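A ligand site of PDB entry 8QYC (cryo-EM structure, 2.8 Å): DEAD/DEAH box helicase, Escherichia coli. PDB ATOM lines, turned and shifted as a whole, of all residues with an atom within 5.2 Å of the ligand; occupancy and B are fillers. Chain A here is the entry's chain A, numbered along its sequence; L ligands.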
ATOM      1  N   ILE A 578      10.997  26.295  10.216  1.00  0.00           N
ATOM      2  CA  ILE A 578       9.878  26.783  11.022  1.00  0.00           C
ATOM      3  C   ILE A 578       9.379  28.076  10.404  1.00  0.00           C
ATOM      4  O   ILE A 578      10.150  29.029  10.204  1.00  0.00           O
ATOM      5  CB  ILE A 578      10.296  27.007  12.489  1.00  0.00           C
ATOM      6  CG1 ILE A 578      10.712  25.678  13.132  1.00  0.00           C
ATOM      7  CG2 ILE A 578       9.173  27.658  13.264  1.00  0.00           C
ATOM      8  CD1 ILE A 578       9.615  24.639  13.140  1.00  0.00           C
ATOM      9  N   ARG A 579       8.080  28.117  10.086  1.00  0.00           N
ATOM     10  CA  ARG A 579       7.440  29.302   9.550  1.00  0.00           C
ATOM     11  C   ARG A 579       6.360  29.774  10.511  1.00  0.00           C
ATOM     12  O   ARG A 579       5.509  28.987  10.927  1.00  0.00           O
ATOM     13  CB  ARG A 579       6.820  29.042   8.169  1.00  0.00           C
ATOM     14  CG  ARG A 579       7.764  29.233   7.004  1.00  0.00           C
ATOM     15  CD  ARG A 579       8.701  28.057   6.831  1.00  0.00           C
ATOM     16  NE  ARG A 579       9.637  28.259   5.733  1.00  0.00           N
ATOM     17  CZ  ARG A 579      10.446  27.328   5.247  1.00  0.00           C
ATOM     18  NH1 ARG A 579      10.443  26.101   5.739  1.00  0.00           N
ATOM     19  NH2 ARG A 579      11.262  27.632   4.247  1.00  0.00           N
ATOM     20  N   LEU A 580       6.401  31.056  10.864  1.00  0.00           N
ATOM     21  CA  LEU A 580       5.343  31.635  11.677  1.00  0.00           C
ATOM     22  C   LEU A 580       4.070  31.792  10.839  1.00  0.00           C
ATOM     23  O   LEU A 580       4.123  32.117   9.659  1.00  0.00           O
ATOM     24  CB  LEU A 580       5.763  32.994  12.225  1.00  0.00           C
ATOM     25  CG  LEU A 580       6.883  33.046  13.262  1.00  0.00           C
ATOM     26  CD1 LEU A 580       7.084  34.473  13.728  1.00  0.00           C
ATOM     27  CD2 LEU A 580       6.551  32.160  14.439  1.00  0.00           C
ATOM     28  N   LYS A 581       2.929  31.553  11.475  1.00  0.00           N
ATOM     29  CA  LYS A 581       1.662  31.781  10.808  1.00  0.00           C
ATOM     30  C   LYS A 581       1.429  33.282  10.652  1.00  0.00           C
ATOM     31  O   LYS A 581       2.138  34.115  11.214  1.00  0.00           O
ATOM     32  CB  LYS A 581       0.511  31.138  11.594  1.00  0.00           C
ATOM     33  CG  LYS A 581       0.743  29.688  11.943  1.00  0.00           C
ATOM     34  CD  LYS A 581       1.048  28.853  10.711  1.00  0.00           C
ATOM     35  CE  LYS A 581       1.348  27.411  11.070  1.00  0.00           C
ATOM     36  NZ  LYS A 581       1.736  26.612   9.875  1.00  0.00           N
ATOM     37  N   GLN A 584       0.598  34.637  13.889  1.00  0.00           N
ATOM     38  CA  GLN A 584       1.794  34.645  14.730  1.00  0.00           C
ATOM     39  C   GLN A 584       2.725  35.783  14.339  1.00  0.00           C
ATOM     40  O   GLN A 584       3.315  36.433  15.214  1.00  0.00           O
ATOM     41  CB  GLN A 584       2.506  33.304  14.642  1.00  0.00           C
ATOM     42  CG  GLN A 584       1.692  32.157  15.194  1.00  0.00           C
ATOM     43  CD  GLN A 584       2.518  30.919  15.423  1.00  0.00           C
ATOM     44  OE1 GLN A 584       3.401  30.583  14.629  1.00  0.00           O
ATOM     45  NE2 GLN A 584       2.231  30.218  16.512  1.00  0.00           N
ATOM     46  N   ASP A 610      -6.579  32.637  22.148  1.00  0.00           N
ATOM     47  CA  ASP A 610      -7.089  31.335  22.570  1.00  0.00           C
ATOM     48  C   ASP A 610      -5.979  30.291  22.558  1.00  0.00           C
ATOM     49  O   ASP A 610      -4.910  30.482  21.954  1.00  0.00           O
ATOM     50  CB  ASP A 610      -8.241  30.893  21.670  1.00  0.00           C
ATOM     51  CG  ASP A 610      -9.561  31.517  22.065  1.00  0.00           C
ATOM     52  OD1 ASP A 610      -9.594  32.254  23.076  1.00  0.00           O
ATOM     53  OD2 ASP A 610     -10.568  31.263  21.370  1.00  0.00           O
ATOM     54  N   MET A 611      -6.224  29.188  23.252  1.00  0.00           N
ATOM     55  CA  MET A 611      -5.271  28.090  23.278  1.00  0.00           C
ATOM     56  C   MET A 611      -5.160  27.450  21.910  1.00  0.00           C
ATOM     57  O   MET A 611      -6.138  27.364  21.151  1.00  0.00           O
ATOM     58  CB  MET A 611      -5.688  27.047  24.317  1.00  0.00           C
ATOM     59  CG  MET A 611      -5.548  27.501  25.761  1.00  0.00           C
ATOM     60  SD  MET A 611      -3.836  27.694  26.295  1.00  0.00           S
ATOM     61  CE  MET A 611      -3.643  29.467  26.214  1.00  0.00           C
ATOM     62  N   GLY A 612      -3.957  26.999  21.584  1.00  0.00           N
ATOM     63  CA  GLY A 612      -3.684  26.392  20.301  1.00  0.00           C
ATOM     64  C   GLY A 612      -3.313  27.352  19.199  1.00  0.00           C
ATOM     65  O   GLY A 612      -3.188  26.923  18.048  1.00  0.00           O
ATOM     66  N   LEU A 613      -3.114  28.637  19.510  1.00  0.00           N
ATOM     67  CA  LEU A 613      -2.701  29.620  18.522  1.00  0.00           C
ATOM     68  C   LEU A 613      -1.192  29.847  18.534  1.00  0.00           C
ATOM     69  O   LEU A 613      -0.716  30.769  17.859  1.00  0.00           O
ATOM     70  CB  LEU A 613      -3.421  30.952  18.749  1.00  0.00           C
ATOM     71  CG  LEU A 613      -4.955  30.973  18.633  1.00  0.00           C
ATOM     72  CD1 LEU A 613      -5.424  32.382  18.296  1.00  0.00           C
ATOM     73  CD2 LEU A 613      -5.452  29.971  17.613  1.00  0.00           C
ATOM     74  N   GLY A 614      -0.449  29.040  19.278  1.00  0.00           N
ATOM     75  CA  GLY A 614       0.992  29.208  19.340  1.00  0.00           C
ATOM     76  C   GLY A 614       1.443  30.480  20.022  1.00  0.00           C
ATOM     77  O   GLY A 614       2.361  31.153  19.515  1.00  0.00           O
ATOM     78  N   LYS A 615       0.828  30.841  21.151  1.00  0.00           N
ATOM     79  CA  LYS A 615       1.271  32.014  21.892  1.00  0.00           C
ATOM     80  C   LYS A 615       2.695  31.820  22.404  1.00  0.00           C
ATOM     81  O   LYS A 615       3.474  32.782  22.475  1.00  0.00           O
ATOM     82  CB  LYS A 615       0.321  32.291  23.053  1.00  0.00           C
ATOM     83  CG  LYS A 615      -1.082  32.694  22.620  1.00  0.00           C
ATOM     84  CD  LYS A 615      -2.062  32.520  23.765  1.00  0.00           C
ATOM     85  CE  LYS A 615      -1.652  33.313  24.982  1.00  0.00           C
ATOM     86  NZ  LYS A 615      -2.602  33.103  26.105  1.00  0.00           N
ATOM     87  N   THR A 616       3.040  30.584  22.791  1.00  0.00           N
ATOM     88  CA  THR A 616       4.392  30.311  23.259  1.00  0.00           C
ATOM     89  C   THR A 616       5.421  30.639  22.180  1.00  0.00           C
ATOM     90  O   THR A 616       6.444  31.265  22.479  1.00  0.00           O
ATOM     91  CB  THR A 616       4.511  28.840  23.665  1.00  0.00           C
ATOM     92  OG1 THR A 616       3.646  28.584  24.779  1.00  0.00           O
ATOM     93  CG2 THR A 616       5.937  28.513  24.063  1.00  0.00           C
ATOM     94  N   LEU A 617       5.150  30.258  20.941  1.00  0.00           N
ATOM     95  CA  LEU A 617       6.086  30.552  19.858  1.00  0.00           C
ATOM     96  C   LEU A 617       6.178  32.058  19.585  1.00  0.00           C
ATOM     97  O   LEU A 617       7.268  32.570  19.318  1.00  0.00           O
ATOM     98  CB  LEU A 617       5.688  29.808  18.588  1.00  0.00           C
ATOM     99  CG  LEU A 617       6.611  29.972  17.376  1.00  0.00           C
ATOM    100  CD1 LEU A 617       8.062  29.732  17.771  1.00  0.00           C
ATOM    101  CD2 LEU A 617       6.202  29.036  16.268  1.00  0.00           C
ATOM    102  N   LEU A 644       4.346  23.866  32.446  1.00  0.00           N
ATOM    103  CA  LEU A 644       4.505  24.770  31.316  1.00  0.00           C
ATOM    104  C   LEU A 644       5.936  25.254  31.157  1.00  0.00           C
ATOM    105  O   LEU A 644       6.326  25.622  30.037  1.00  0.00           O
ATOM    106  CB  LEU A 644       3.572  25.966  31.457  1.00  0.00           C
ATOM    107  CG  LEU A 644       2.079  25.625  31.487  1.00  0.00           C
ATOM    108  CD1 LEU A 644       1.262  26.882  31.372  1.00  0.00           C
ATOM    109  CD2 LEU A 644       1.727  24.649  30.378  1.00  0.00           C
ATOM    110  N   ASN A 647       7.513  22.828  28.901  1.00  0.00           N
ATOM    111  CA  ASN A 647       7.080  23.074  27.528  1.00  0.00           C
ATOM    112  C   ASN A 647       7.784  24.291  26.932  1.00  0.00           C
ATOM    113  O   ASN A 647       8.133  24.291  25.753  1.00  0.00           O
ATOM    114  CB  ASN A 647       5.562  23.275  27.491  1.00  0.00           C
ATOM    115  CG  ASN A 647       5.037  23.475  26.093  1.00  0.00           C
ATOM    116  OD1 ASN A 647       4.747  22.520  25.377  1.00  0.00           O
ATOM    117  ND2 ASN A 647       4.902  24.736  25.681  1.00  0.00           N
ATOM    118  N   TRP A 648       8.002  25.330  27.741  1.00  0.00           N
ATOM    119  CA  TRP A 648       8.694  26.519  27.252  1.00  0.00           C
ATOM    120  C   TRP A 648      10.123  26.191  26.837  1.00  0.00           C
ATOM    121  O   TRP A 648      10.569  26.560  25.752  1.00  0.00           O
ATOM    122  CB  TRP A 648       8.693  27.607  28.335  1.00  0.00           C
ATOM    123  CG  TRP A 648       7.504  28.512  28.250  1.00  0.00           C
ATOM    124  CD1 TRP A 648       6.312  28.353  28.886  1.00  0.00           C
ATOM    125  CD2 TRP A 648       7.396  29.707  27.477  1.00  0.00           C
ATOM    126  NE1 TRP A 648       5.469  29.380  28.556  1.00  0.00           N
ATOM    127  CE2 TRP A 648       6.114  30.222  27.695  1.00  0.00           C
ATOM    128  CE3 TRP A 648       8.273  30.386  26.625  1.00  0.00           C
ATOM    129  CZ2 TRP A 648       5.676  31.403  27.093  1.00  0.00           C
ATOM    130  CZ3 TRP A 648       7.834  31.547  26.032  1.00  0.00           C
ATOM    131  CH2 TRP A 648       6.553  32.042  26.260  1.00  0.00           C
ATOM    132  N   GLU A 651      10.029  23.951  23.624  1.00  0.00           N
ATOM    133  CA  GLU A 651       9.744  24.668  22.387  1.00  0.00           C
ATOM    134  C   GLU A 651      10.849  25.644  22.025  1.00  0.00           C
ATOM    135  O   GLU A 651      11.097  25.874  20.838  1.00  0.00           O
ATOM    136  CB  GLU A 651       8.396  25.388  22.491  1.00  0.00           C
ATOM    137  CG  GLU A 651       7.210  24.446  22.660  1.00  0.00           C
ATOM    138  CD  GLU A 651       5.894  25.078  22.243  1.00  0.00           C
ATOM    139  OE1 GLU A 651       5.925  26.026  21.441  1.00  0.00           O
ATOM    140  OE2 GLU A 651       4.846  24.620  22.731  1.00  0.00           O
ATOM    141  N   PHE A 655      12.330  25.192  18.287  1.00  0.00           N
ATOM    142  CA  PHE A 655      12.131  26.199  17.248  1.00  0.00           C
ATOM    143  C   PHE A 655      13.355  27.064  16.978  1.00  0.00           C
ATOM    144  O   PHE A 655      13.450  27.634  15.893  1.00  0.00           O
ATOM    145  CB  PHE A 655      10.954  27.113  17.602  1.00  0.00           C
ATOM    146  CG  PHE A 655       9.618  26.420  17.581  1.00  0.00           C
ATOM    147  CD1 PHE A 655       9.065  25.986  16.390  1.00  0.00           C
ATOM    148  CD2 PHE A 655       8.901  26.240  18.746  1.00  0.00           C
ATOM    149  CE1 PHE A 655       7.838  25.365  16.369  1.00  0.00           C
ATOM    150  CE2 PHE A 655       7.663  25.611  18.728  1.00  0.00           C
ATOM    151  CZ  PHE A 655       7.141  25.172  17.536  1.00  0.00           C
ATOM    152  N   ASP A 730       2.904  33.409  32.133  1.00  0.00           N
ATOM    153  CA  ASP A 730       2.041  32.481  31.416  1.00  0.00           C
ATOM    154  C   ASP A 730       0.926  31.984  32.325  1.00  0.00           C
ATOM    155  O   ASP A 730       1.125  31.779  33.523  1.00  0.00           O
ATOM    156  CB  ASP A 730       2.858  31.305  30.892  1.00  0.00           C
ATOM    157  CG  ASP A 730       4.033  31.751  30.056  1.00  0.00           C
ATOM    158  OD1 ASP A 730       3.827  32.607  29.170  1.00  0.00           O
ATOM    159  OD2 ASP A 730       5.155  31.263  30.303  1.00  0.00           O
ATOM    160  N   GLU A 731      -0.250  31.791  31.731  1.00  0.00           N
ATOM    161  CA  GLU A 731      -1.472  31.535  32.488  1.00  0.00           C
ATOM    162  C   GLU A 731      -1.636  32.590  33.581  1.00  0.00           C
ATOM    163  O   GLU A 731      -1.645  32.299  34.779  1.00  0.00           O
ATOM    164  CB  GLU A 731      -1.488  30.118  33.068  1.00  0.00           C
ATOM    165  CG  GLU A 731      -1.424  29.040  32.006  1.00  0.00           C
ATOM    166  CD  GLU A 731      -2.459  29.218  30.913  1.00  0.00           C
ATOM    167  OE1 GLU A 731      -3.639  29.482  31.242  1.00  0.00           O
ATOM    168  OE2 GLU A 731      -2.088  29.101  29.730  1.00  0.00           O
ATOM    169  N   ARG A1021      -5.520  21.142  15.722  1.00  0.00           N
ATOM    170  CA  ARG A1021      -4.282  21.772  16.182  1.00  0.00           C
ATOM    171  C   ARG A1021      -3.486  22.242  14.977  1.00  0.00           C
ATOM    172  O   ARG A1021      -3.809  21.931  13.832  1.00  0.00           O
ATOM    173  CB  ARG A1021      -3.424  20.813  16.996  1.00  0.00           C
ATOM    174  CG  ARG A1021      -3.909  20.563  18.407  1.00  0.00           C
ATOM    175  CD  ARG A1021      -3.077  19.487  19.075  1.00  0.00           C
ATOM    176  NE  ARG A1021      -1.679  19.875  19.184  1.00  0.00           N
ATOM    177  CZ  ARG A1021      -1.160  20.518  20.230  1.00  0.00           C
ATOM    178  NH1 ARG A1021      -1.906  20.861  21.264  1.00  0.00           N
ATOM    179  NH2 ARG A1021       0.142  20.811  20.229  1.00  0.00           N
ATOM    180  N   ILE A1022      -2.436  23.005  15.254  1.00  0.00           N
ATOM    181  CA  ILE A1022      -1.416  23.305  14.260  1.00  0.00           C
ATOM    182  C   ILE A1022      -0.567  22.052  14.058  1.00  0.00           C
ATOM    183  O   ILE A1022      -0.037  21.495  15.023  1.00  0.00           O
ATOM    184  CB  ILE A1022      -0.562  24.498  14.688  1.00  0.00           C
ATOM    185  CG1 ILE A1022      -1.440  25.735  14.909  1.00  0.00           C
ATOM    186  CG2 ILE A1022       0.521  24.787  13.663  1.00  0.00           C
ATOM    187  CD1 ILE A1022      -0.678  26.954  15.369  1.00  0.00           C
HETATM  188  P1  LIG L   1       0.195  28.074  25.844  1.00  0.00           P
HETATM  189  S1  LIG L   1       0.976  29.847  26.044  1.00  0.00           S
HETATM  190  O1  LIG L   1      -0.451  27.639  27.191  1.00  0.00           O
HETATM  191  O2  LIG L   1       1.313  27.059  25.462  1.00  0.00           O
HETATM  192  P2  LIG L   1      -0.479  28.187  23.194  1.00  0.00           P
HETATM  193  O3  LIG L   1      -1.067  29.394  22.579  1.00  0.00           O
HETATM  194  O4  LIG L   1       1.056  28.196  23.174  1.00  0.00           O
HETATM  195  O5  LIG L   1      -0.898  28.079  24.728  1.00  0.00           O
HETATM  196  P3  LIG L   1       0.178  25.820  21.982  1.00  0.00           P
HETATM  197  O6  LIG L   1       1.543  26.275  22.306  1.00  0.00           O
HETATM  198  O7  LIG L   1      -0.216  24.519  22.682  1.00  0.00           O
HETATM  199  O8  LIG L   1      -0.925  26.883  22.414  1.00  0.00           O
HETATM  200  O9  LIG L   1       0.067  25.664  20.407  1.00  0.00           O
HETATM  201  C1  LIG L   1      -0.205  24.381  19.814  1.00  0.00           C
HETATM  202  C2  LIG L   1       1.030  23.843  19.125  1.00  0.00           C
HETATM  203  O10 LIG L   1       1.211  24.500  17.869  1.00  0.00           O
HETATM  204  C3  LIG L   1       2.350  24.053  19.851  1.00  0.00           C
HETATM  205  O11 LIG L   1       2.591  23.008  20.779  1.00  0.00           O
HETATM  206  C4  LIG L   1       3.387  24.055  18.709  1.00  0.00           C
HETATM  207  O12 LIG L   1       4.064  22.812  18.628  1.00  0.00           O
HETATM  208  C5  LIG L   1       2.537  24.281  17.441  1.00  0.00           C
HETATM  209  N1  LIG L   1       2.955  25.426  16.640  1.00  0.00           N
HETATM  210  C6  LIG L   1       2.725  26.755  16.895  1.00  0.00           C
HETATM  211  N2  LIG L   1       3.209  27.553  15.989  1.00  0.00           N
HETATM  212  C7  LIG L   1       3.798  26.710  15.063  1.00  0.00           C
HETATM  213  C8  LIG L   1       4.490  26.944  13.858  1.00  0.00           C
HETATM  214  N3  LIG L   1       4.713  28.163  13.357  1.00  0.00           N
HETATM  215  N4  LIG L   1       4.953  25.869  13.182  1.00  0.00           N
HETATM  216  C9  LIG L   1       4.730  24.650  13.683  1.00  0.00           C
HETATM  217  N5  LIG L   1       4.096  24.304  14.800  1.00  0.00           N
HETATM  218  C10 LIG L   1       3.647  25.386  15.451  1.00  0.00           C
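A nitrogen (N3) of the ligand is in hydrogen-bond range of the backbone carbonyl oxygen (O) of Arg 579 (2.7 Å). O3 of the ligand sits at hydrogen-bond distance from N of Lys 615, 2.8 Å away. O4 of the ligand lies within hydrogen-bond range of N of Thr 616, 3.1 Å away. An oxygen (O2) of the ligand sits at hydrogen-bond distance from the side-chain hydroxyl (OG1) of Thr 616 (2.9 Å). The side-chain amide nitrogen (NE2) of Gln 584 sits at hydrogen-bond distance from a nitrogen (N2) of the ligand (2.9 Å). The backbone NH of Gly 612 lies within hydrogen-bond range of an oxygen (O8) of the ligand (3.1 Å). O11 of the ligand lies within hydrogen-bond range of NH2 of Arg 1021. SD of Met 611 is in hydrogen-bond range of O1 of the ligand (3.5 Å). OE2 of Glu 731 is in hydrogen-bond range of O1 of the ligand, 3.4 Å away. An oxygen (O3) of the ligand lies within hydrogen-bond range of the backbone NH (N) of Gly 614 (3.4 Å). O11 of the ligand is in hydrogen-bond range of OE2 of Glu 651, at 3.4 Å.
NE2 of Gln 584 lies within hydrogen-bond range of O of Gly 614, 3.1 Å away. The side-chain amide nitrogen (NE2) of Gln 584 lies within hydrogen-bond range of the backbone carbonyl oxygen (O) of Leu 613 (3.3 Å). N of Lys 581 lies within hydrogen-bond range of OE1 of Gln 584 (3.3 Å). OE2 of Glu 651 is in hydrogen-bond range of ND2 of Asn 647, at 3.0 Å.
Leu 580 touches the ligand. Leu 613 touches the ligand. CD2 of Leu 617 touches N2 of the ligand, at 3.4 Å. Ile 1022 touches the ligand (CB to O10, 3.6 Å). Hydrophobic or aromatic side chains within 4 Å of the ligand: Met 611, Leu 617 and Ile 1022. 14 residues have an atom within 4 Å of the ligand: Arg 579, Leu 580, Gln 584, Met 611, Gly 612, Leu 613, Gly 614, Lys 615, Thr 616, Leu 617, Glu 651, Glu 731, Arg 1021 and Ile 1022.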
